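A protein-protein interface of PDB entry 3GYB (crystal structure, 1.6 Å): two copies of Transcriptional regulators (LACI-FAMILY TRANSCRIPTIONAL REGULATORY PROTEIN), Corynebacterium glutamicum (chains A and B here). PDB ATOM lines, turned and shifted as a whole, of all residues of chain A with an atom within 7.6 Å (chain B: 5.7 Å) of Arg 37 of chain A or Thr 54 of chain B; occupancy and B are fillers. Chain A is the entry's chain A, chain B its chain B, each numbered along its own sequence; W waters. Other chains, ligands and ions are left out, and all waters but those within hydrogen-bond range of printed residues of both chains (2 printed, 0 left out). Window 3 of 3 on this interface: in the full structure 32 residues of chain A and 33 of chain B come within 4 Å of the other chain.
N of Arg 37 of chain A lies within hydrogen-bond range of O of Gln 6 of chain A, 2.8 Å away.
N of Asp 62 of chain A is in hydrogen-bond range of O of Leu 7 of chain A (2.7 Å).
N of Ile 8 of chain A sits at hydrogen-bond distance from O of Arg 37 of chain A (2.9 Å).
O of Ser 28 of chain A sits at hydrogen-bond distance from OG1 of Thr 32 of chain A.
The side-chain hydroxyl (OG) of Ser 55 of chain B lies within hydrogen-bond range of the side-chain amide oxygen (OE1) of Gln 47 of chain B, at 2.7 Å.
The backbone carbonyl oxygen (O) of Ser 55 of chain B lies within hydrogen-bond range of the side-chain hydroxyl (OG) of Ser 58 of chain B (2.5 Å).
Among the printed residues, pairs that only touch across the chains: Leu 7 of chain A with Ser 58 of chain B (2.9 Å), Thr 32 of chain A with Gln 47 of chain B (3.9 Å), Arg 37 of chain A with Ser 46 of chain B (3.1 Å), Arg 37 of chain A with Gln 47 of chain B (3.5 Å) and Arg 37 of chain A with Thr 54 of chain B (3.9 Å).
NH2 of Arg 37 of chain A is in salt-bridge range of OD2 of Asp 51 of chain B, at 2.8 Å.
The guanidinium group (NH1) of Arg 37 of chain A is in hydrogen-bond range of the side-chain hydroxyl (OG) of Ser 55 of chain B, 2.8 Å away.
OG of Ser 46 of chain B lies within hydrogen-bond range of O of Leu 38 of chain A (2.7 Å).
Of the 19 printed residues of chain A, 4 touch a printed residue of chain B.
Printed residues of chain A that touch a printed residue of chain B: Leu 7, Thr 32, Arg 37 and Leu 38.
Among the printed residues, 8 pairs touch across the chains.
No position is printed for both chains.
Of chain B, only Ser 46 (3.1 Å), Gln 47 (3.5 Å), Asp 51 (2.8 Å), Thr 54 (3.9 Å) and Ser 55 (2.8 Å) come within 4 Å of Arg 37 of chain A.
Of the printed residues of chain A, Asp 51 of chain B touches Arg 37.
Of chain A, only Arg 37 comes within 4 Å of Thr 54 of chain B.
Printed residues of chain A within 4 Å of Ser 55 of chain B: Arg 37 (2.8 Å).
The nearest residue of chain A that does not touch Thr 54 of chain B is Leu 7 of chain A (6.4 Å).
The nearest printed residue of chain A that does not touch Ser 55 of chain B is Leu 7 of chain A (4.1 Å).
Water W2 lies within hydrogen-bond range of O of Thr 5 of chain A and OG of Ser 58 of chain B.
Water W1 bridges O of Ser 58 of chain B (2.7 Å) and O of Met 59 of chain A (2.9 Å).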
ATOM      1  N   THR A   5      -1.691  -3.504 -23.903  1.00  0.00           N
ATOM      2  CA  THR A   5      -0.386  -2.858 -23.856  1.00  0.00           C
ATOM      3  C   THR A   5      -0.199  -1.796 -24.938  1.00  0.00           C
ATOM      4  O   THR A   5       0.753  -1.017 -24.885  1.00  0.00           O
ATOM      5  CB  THR A   5       0.734  -3.901 -24.002  1.00  0.00           C
ATOM      6  OG1 THR A   5       0.602  -4.565 -25.266  1.00  0.00           O
ATOM      7  CG2 THR A   5       0.643  -4.936 -22.886  1.00  0.00           C
ATOM      8  N   GLN A   6      -1.106  -1.769 -25.912  1.00  0.00           N
ATOM      9  CA  GLN A   6      -1.035  -0.814 -27.017  1.00  0.00           C
ATOM     10  C   GLN A   6       0.198  -1.093 -27.860  1.00  0.00           C
ATOM     11  O   GLN A   6       0.657  -0.247 -28.628  1.00  0.00           O
ATOM     12  CB  GLN A   6      -0.976   0.617 -26.489  1.00  0.00           C
ATOM     13  CG  GLN A   6      -2.259   1.077 -25.825  1.00  0.00           C
ATOM     14  CD  GLN A   6      -2.204   2.533 -25.414  1.00  0.00           C
ATOM     15  OE1 GLN A   6      -1.432   2.911 -24.532  1.00  0.00           O
ATOM     16  NE2 GLN A   6      -3.021   3.360 -26.057  1.00  0.00           N
ATOM     17  N   LEU A   7       0.727  -2.298 -27.703  1.00  0.00           N
ATOM     18  CA  LEU A   7       1.907  -2.717 -28.429  1.00  0.00           C
ATOM     19  C   LEU A   7       1.555  -3.622 -29.599  1.00  0.00           C
ATOM     20  O   LEU A   7       0.701  -4.502 -29.484  1.00  0.00           O
ATOM     21  CB  LEU A   7       2.848  -3.452 -27.479  1.00  0.00           C
ATOM     22  CG  LEU A   7       3.684  -2.622 -26.504  1.00  0.00           C
ATOM     23  CD1 LEU A   7       4.344  -3.545 -25.475  1.00  0.00           C
ATOM     24  CD2 LEU A   7       4.730  -1.827 -27.280  1.00  0.00           C
ATOM     25  N   ILE A   8       2.202  -3.380 -30.733  1.00  0.00           N
ATOM     26  CA  ILE A   8       1.996  -4.190 -31.923  1.00  0.00           C
ATOM     27  C   ILE A   8       3.365  -4.718 -32.317  1.00  0.00           C
ATOM     28  O   ILE A   8       4.294  -3.940 -32.530  1.00  0.00           O
ATOM     29  CB  ILE A   8       1.424  -3.359 -33.099  1.00  0.00           C
ATOM     30  CG1 ILE A   8       0.046  -2.803 -32.733  1.00  0.00           C
ATOM     31  CG2 ILE A   8       1.339  -4.222 -34.354  1.00  0.00           C
ATOM     32  CD1 ILE A   8      -1.004  -3.868 -32.473  1.00  0.00           C
ATOM     33  N   ALA A   9       3.494  -6.038 -32.384  1.00  0.00           N
ATOM     34  CA  ALA A   9       4.755  -6.663 -32.763  1.00  0.00           C
ATOM     35  C   ALA A   9       4.774  -6.818 -34.278  1.00  0.00           C
ATOM     36  O   ALA A   9       3.787  -7.237 -34.877  1.00  0.00           O
ATOM     37  CB  ALA A   9       4.885  -8.030 -32.093  1.00  0.00           C
ATOM     38  N   VAL A  10       5.896  -6.469 -34.896  1.00  0.00           N
ATOM     39  CA  VAL A  10       6.027  -6.586 -36.338  1.00  0.00           C
ATOM     40  C   VAL A  10       7.167  -7.554 -36.636  1.00  0.00           C
ATOM     41  O   VAL A  10       8.314  -7.308 -36.258  1.00  0.00           O
ATOM     42  CB  VAL A  10       6.326  -5.213 -36.978  1.00  0.00           C
ATOM     43  CG1 VAL A  10       6.393  -5.350 -38.493  1.00  0.00           C
ATOM     44  CG2 VAL A  10       5.243  -4.214 -36.584  1.00  0.00           C
ATOM     45  N   SER A  28       2.900   2.324 -39.384  1.00  0.00           N
ATOM     46  CA  SER A  28       3.043   3.304 -38.317  1.00  0.00           C
ATOM     47  C   SER A  28       2.138   4.516 -38.494  1.00  0.00           C
ATOM     48  O   SER A  28       1.515   4.982 -37.537  1.00  0.00           O
ATOM     49  CB  SER A  28       4.501   3.766 -38.225  1.00  0.00           C
ATOM     50  OG  SER A  28       4.652   4.746 -37.211  1.00  0.00           O
ATOM     51  N   LEU A  31      -1.307   3.262 -37.412  1.00  0.00           N
ATOM     52  CA  LEU A  31      -1.427   2.824 -36.023  1.00  0.00           C
ATOM     53  C   LEU A  31      -0.991   3.761 -34.898  1.00  0.00           C
ATOM     54  O   LEU A  31      -1.681   3.858 -33.884  1.00  0.00           O
ATOM     55  CB  LEU A  31      -0.706   1.483 -35.852  1.00  0.00           C
ATOM     56  CG  LEU A  31      -1.235   0.343 -36.724  1.00  0.00           C
ATOM     57  CD1 LEU A  31      -0.356  -0.888 -36.564  1.00  0.00           C
ATOM     58  CD2 LEU A  31      -2.673   0.035 -36.333  1.00  0.00           C
ATOM     59  N   THR A  32       0.135   4.450 -35.057  1.00  0.00           N
ATOM     60  CA  THR A  32       0.613   5.317 -33.983  1.00  0.00           C
ATOM     61  C   THR A  32      -0.291   6.495 -33.618  1.00  0.00           C
ATOM     62  O   THR A  32      -0.371   6.873 -32.450  1.00  0.00           O
ATOM     63  CB  THR A  32       2.055   5.816 -34.255  1.00  0.00           C
ATOM     64  OG1 THR A  32       2.103   6.551 -35.483  1.00  0.00           O
ATOM     65  CG2 THR A  32       3.005   4.626 -34.344  1.00  0.00           C
ATOM     66  N   LYS A  34      -3.226   6.450 -33.306  1.00  0.00           N
ATOM     67  CA  LYS A  34      -4.270   5.867 -32.473  1.00  0.00           C
ATOM     68  C   LYS A  34      -3.771   5.390 -31.111  1.00  0.00           C
ATOM     69  O   LYS A  34      -4.521   4.781 -30.351  1.00  0.00           O
ATOM     70  CB  LYS A  34      -4.942   4.710 -33.213  1.00  0.00           C
ATOM     71  CG  LYS A  34      -5.745   5.143 -34.428  1.00  0.00           C
ATOM     72  CD  LYS A  34      -6.323   3.945 -35.161  1.00  0.00           C
ATOM     73  CE  LYS A  34      -7.226   4.377 -36.305  1.00  0.00           C
ATOM     74  NZ  LYS A  34      -8.424   5.120 -35.819  1.00  0.00           N
ATOM     75  N   GLY A  35      -2.505   5.656 -30.811  1.00  0.00           N
ATOM     76  CA  GLY A  35      -1.963   5.263 -29.523  1.00  0.00           C
ATOM     77  C   GLY A  35      -1.128   3.999 -29.492  1.00  0.00           C
ATOM     78  O   GLY A  35      -0.598   3.636 -28.447  1.00  0.00           O
ATOM     79  N   TYR A  36      -1.002   3.322 -30.626  1.00  0.00           N
ATOM     80  CA  TYR A  36      -0.211   2.098 -30.667  1.00  0.00           C
ATOM     81  C   TYR A  36       1.266   2.401 -30.854  1.00  0.00           C
ATOM     82  O   TYR A  36       1.634   3.430 -31.422  1.00  0.00           O
ATOM     83  CB  TYR A  36      -0.689   1.193 -31.805  1.00  0.00           C
ATOM     84  CG  TYR A  36      -2.039   0.564 -31.548  1.00  0.00           C
ATOM     85  CD1 TYR A  36      -2.169  -0.519 -30.679  1.00  0.00           C
ATOM     86  CD2 TYR A  36      -3.191   1.076 -32.142  1.00  0.00           C
ATOM     87  CE1 TYR A  36      -3.415  -1.077 -30.406  1.00  0.00           C
ATOM     88  CE2 TYR A  36      -4.445   0.528 -31.873  1.00  0.00           C
ATOM     89  CZ  TYR A  36      -4.547  -0.546 -31.006  1.00  0.00           C
ATOM     90  OH  TYR A  36      -5.782  -1.078 -30.727  1.00  0.00           O
ATOM     91  N   ARG A  37       2.100   1.495 -30.356  1.00  0.00           N
ATOM     92  CA  ARG A  37       3.549   1.604 -30.480  1.00  0.00           C
ATOM     93  C   ARG A  37       4.000   0.299 -31.128  1.00  0.00           C
ATOM     94  O   ARG A  37       3.413  -0.753 -30.874  1.00  0.00           O
ATOM     95  CB  ARG A  37       4.186   1.781 -29.103  1.00  0.00           C
ATOM     96  CG  ARG A  37       3.873   3.133 -28.477  1.00  0.00           C
ATOM     97  CD  ARG A  37       4.258   3.193 -27.011  1.00  0.00           C
ATOM     98  NE  ARG A  37       3.865   4.468 -26.411  1.00  0.00           N
ATOM     99  CZ  ARG A  37       4.603   5.573 -26.434  1.00  0.00           C
ATOM    100  NH1 ARG A  37       5.792   5.576 -27.025  1.00  0.00           N
ATOM    101  NH2 ARG A  37       4.143   6.685 -25.879  1.00  0.00           N
ATOM    102  N   LEU A  38       5.037   0.367 -31.956  1.00  0.00           N
ATOM    103  CA  LEU A  38       5.525  -0.811 -32.668  1.00  0.00           C
ATOM    104  C   LEU A  38       6.914  -1.266 -32.261  1.00  0.00           C
ATOM    105  O   LEU A  38       7.768  -0.454 -31.936  1.00  0.00           O
ATOM    106  CB  LEU A  38       5.559  -0.529 -34.171  1.00  0.00           C
ATOM    107  CG  LEU A  38       4.369   0.182 -34.814  1.00  0.00           C
ATOM    108  CD1 LEU A  38       4.664   0.415 -36.289  1.00  0.00           C
ATOM    109  CD2 LEU A  38       3.108  -0.644 -34.642  1.00  0.00           C
ATOM    110  N   SER A  39       7.130  -2.579 -32.294  1.00  0.00           N
ATOM    111  CA  SER A  39       8.438  -3.149 -31.989  1.00  0.00           C
ATOM    112  C   SER A  39       8.667  -4.257 -33.008  1.00  0.00           C
ATOM    113  O   SER A  39       7.745  -5.008 -33.338  1.00  0.00           O
ATOM    114  CB  SER A  39       8.485  -3.714 -30.569  1.00  0.00           C
ATOM    115  OG  SER A  39       9.824  -4.032 -30.215  1.00  0.00           O
ATOM    116  N   MET A  59       6.209  -9.830 -25.311  1.00  0.00           N
ATOM    117  CA  MET A  59       5.949  -8.427 -25.014  1.00  0.00           C
ATOM    118  C   MET A  59       4.457  -8.211 -24.757  1.00  0.00           C
ATOM    119  O   MET A  59       4.023  -7.100 -24.457  1.00  0.00           O
ATOM    120  CB  MET A  59       6.429  -7.524 -26.171  1.00  0.00           C
ATOM    121  CG  MET A  59       5.528  -7.498 -27.397  1.00  0.00           C
ATOM    122  SD  MET A  59       6.076  -6.211 -28.778  1.00  0.00           S
ATOM    123  CE  MET A  59       5.378  -4.651 -28.107  1.00  0.00           C
ATOM    124  N   PRO A  61       1.807  -8.339 -26.876  1.00  0.00           N
ATOM    125  CA  PRO A  61       1.267  -7.373 -27.834  1.00  0.00           C
ATOM    126  C   PRO A  61      -0.244  -7.508 -28.000  1.00  0.00           C
ATOM    127  O   PRO A  61      -0.795  -8.597 -27.834  1.00  0.00           O
ATOM    128  CB  PRO A  61       2.019  -7.720 -29.114  1.00  0.00           C
ATOM    129  CG  PRO A  61       2.116  -9.217 -29.019  1.00  0.00           C
ATOM    130  CD  PRO A  61       2.513  -9.432 -27.571  1.00  0.00           C
ATOM    131  N   ASP A  62      -0.905  -6.399 -28.319  1.00  0.00           N
ATOM    132  CA  ASP A  62      -2.349  -6.408 -28.536  1.00  0.00           C
ATOM    133  C   ASP A  62      -2.623  -7.053 -29.891  1.00  0.00           C
ATOM    134  O   ASP A  62      -3.659  -7.688 -30.094  1.00  0.00           O
ATOM    135  CB  ASP A  62      -2.919  -4.985 -28.542  1.00  0.00           C
ATOM    136  CG  ASP A  62      -2.839  -4.305 -27.186  1.00  0.00           C
ATOM    137  OD1 ASP A  62      -2.536  -4.980 -26.181  1.00  0.00           O
ATOM    138  OD2 ASP A  62      -3.096  -3.085 -27.129  1.00  0.00           O
ATOM    139  N   GLY A  63      -1.682  -6.873 -30.817  1.00  0.00           N
ATOM    140  CA  GLY A  63      -1.813  -7.431 -32.150  1.00  0.00           C
ATOM    141  C   GLY A  63      -0.446  -7.719 -32.741  1.00  0.00           C
ATOM    142  O   GLY A  63       0.570  -7.251 -32.222  1.00  0.00           O
ATOM    143  N   SER B  46       8.317   3.501 -34.537  1.00  0.00           N
ATOM    144  CA  SER B  46       7.812   2.799 -33.361  1.00  0.00           C
ATOM    145  C   SER B  46       6.774   3.570 -32.549  1.00  0.00           C
ATOM    146  O   SER B  46       5.951   2.965 -31.859  1.00  0.00           O
ATOM    147  CB  SER B  46       8.976   2.388 -32.455  1.00  0.00           C
ATOM    148  OG  SER B  46       9.640   1.251 -32.989  1.00  0.00           O
ATOM    149  N   GLN B  47       6.808   4.896 -32.629  1.00  0.00           N
ATOM    150  CA  GLN B  47       5.853   5.716 -31.892  1.00  0.00           C
ATOM    151  C   GLN B  47       5.592   7.040 -32.601  1.00  0.00           C
ATOM    152  O   GLN B  47       6.375   7.464 -33.446  1.00  0.00           O
ATOM    153  CB  GLN B  47       6.350   5.972 -30.462  1.00  0.00           C
ATOM    154  CG  GLN B  47       7.734   6.588 -30.354  1.00  0.00           C
ATOM    155  CD  GLN B  47       8.850   5.601 -30.648  1.00  0.00           C
ATOM    156  OE1 GLN B  47       8.895   4.505 -30.081  1.00  0.00           O
ATOM    157  NE2 GLN B  47       9.770   5.993 -31.524  1.00  0.00           N
ATOM    158  N   ASP B  51       9.415   9.504 -27.799  1.00  0.00           N
ATOM    159  CA  ASP B  51       9.659   8.778 -26.562  1.00  0.00           C
ATOM    160  C   ASP B  51       9.862   7.273 -26.742  1.00  0.00           C
ATOM    161  O   ASP B  51       9.080   6.470 -26.242  1.00  0.00           O
ATOM    162  CB  ASP B  51       8.504   9.038 -25.588  1.00  0.00           C
ATOM    163  CG  ASP B  51       7.144   8.673 -26.171  1.00  0.00           C
ATOM    164  OD1 ASP B  51       7.033   8.511 -27.407  1.00  0.00           O
ATOM    165  OD2 ASP B  51       6.175   8.563 -25.388  1.00  0.00           O
ATOM    166  N   PRO B  52      10.934   6.875 -27.453  1.00  0.00           N
ATOM    167  CA  PRO B  52      11.261   5.466 -27.707  1.00  0.00           C
ATOM    168  C   PRO B  52      11.429   4.652 -26.423  1.00  0.00           C
ATOM    169  O   PRO B  52      11.081   3.468 -26.373  1.00  0.00           O
ATOM    170  CB  PRO B  52      12.566   5.552 -28.501  1.00  0.00           C
ATOM    171  CG  PRO B  52      12.471   6.875 -29.185  1.00  0.00           C
ATOM    172  CD  PRO B  52      11.915   7.761 -28.101  1.00  0.00           C
ATOM    173  N   ILE B  53      11.977   5.281 -25.386  1.00  0.00           N
ATOM    174  CA  ILE B  53      12.181   4.583 -24.124  1.00  0.00           C
ATOM    175  C   ILE B  53      10.848   4.156 -23.519  1.00  0.00           C
ATOM    176  O   ILE B  53      10.751   3.092 -22.912  1.00  0.00           O
ATOM    177  CB  ILE B  53      12.963   5.457 -23.119  1.00  0.00           C
ATOM    178  CG1 ILE B  53      14.350   5.765 -23.689  1.00  0.00           C
ATOM    179  CG2 ILE B  53      13.095   4.735 -21.781  1.00  0.00           C
ATOM    180  CD1 ILE B  53      15.207   6.653 -22.802  1.00  0.00           C
ATOM    181  N   THR B  54       9.818   4.978 -23.691  1.00  0.00           N
ATOM    182  CA  THR B  54       8.504   4.628 -23.167  1.00  0.00           C
ATOM    183  C   THR B  54       7.975   3.414 -23.929  1.00  0.00           C
ATOM    184  O   THR B  54       7.322   2.545 -23.355  1.00  0.00           O
ATOM    185  CB  THR B  54       7.516   5.786 -23.316  1.00  0.00           C
ATOM    186  OG1 THR B  54       7.963   6.895 -22.526  1.00  0.00           O
ATOM    187  CG2 THR B  54       6.132   5.363 -22.850  1.00  0.00           C
ATOM    188  N   SER B  55       8.262   3.356 -25.227  1.00  0.00           N
ATOM    189  CA  SER B  55       7.834   2.224 -26.042  1.00  0.00           C
ATOM    190  C   SER B  55       8.564   0.978 -25.539  1.00  0.00           C
ATOM    191  O   SER B  55       7.969  -0.089 -25.399  1.00  0.00           O
ATOM    192  CB  SER B  55       8.182   2.454 -27.513  1.00  0.00           C
ATOM    193  OG  SER B  55       7.467   3.553 -28.048  1.00  0.00           O
ATOM    194  N   ALA B  56       9.859   1.121 -25.273  1.00  0.00           N
ATOM    195  CA  ALA B  56      10.659   0.004 -24.787  1.00  0.00           C
ATOM    196  C   ALA B  56      10.119  -0.529 -23.464  1.00  0.00           C
ATOM    197  O   ALA B  56      10.016  -1.740 -23.270  1.00  0.00           O
ATOM    198  CB  ALA B  56      12.116   0.433 -24.624  1.00  0.00           C
ATOM    199  N   LEU B  57       9.773   0.379 -22.559  1.00  0.00           N
ATOM    200  CA  LEU B  57       9.254  -0.012 -21.255  1.00  0.00           C
ATOM    201  C   LEU B  57       7.916  -0.756 -21.304  1.00  0.00           C
ATOM    202  O   LEU B  57       7.634  -1.576 -20.431  1.00  0.00           O
ATOM    203  CB  LEU B  57       9.110   1.224 -20.355  1.00  0.00           C
ATOM    204  CG  LEU B  57      10.408   1.918 -19.929  1.00  0.00           C
ATOM    205  CD1 LEU B  57      10.094   3.171 -19.119  1.00  0.00           C
ATOM    206  CD2 LEU B  57      11.248   0.956 -19.109  1.00  0.00           C
ATOM    207  N   SER B  58       7.103  -0.485 -22.321  1.00  0.00           N
ATOM    208  CA  SER B  58       5.799  -1.126 -22.420  1.00  0.00           C
ATOM    209  C   SER B  58       5.858  -2.635 -22.596  1.00  0.00           C
ATOM    210  O   SER B  58       4.858  -3.322 -22.378  1.00  0.00           O
ATOM    211  CB  SER B  58       4.972  -0.523 -23.557  1.00  0.00           C
ATOM    212  OG  SER B  58       5.613  -0.663 -24.808  1.00  0.00           O
HETATM  213  O   HOH W   1       4.191  -5.908 -21.818  1.00  0.00           O
HETATM  214  O   HOH W   2       2.830   0.596 -25.541  1.00  0.00           O
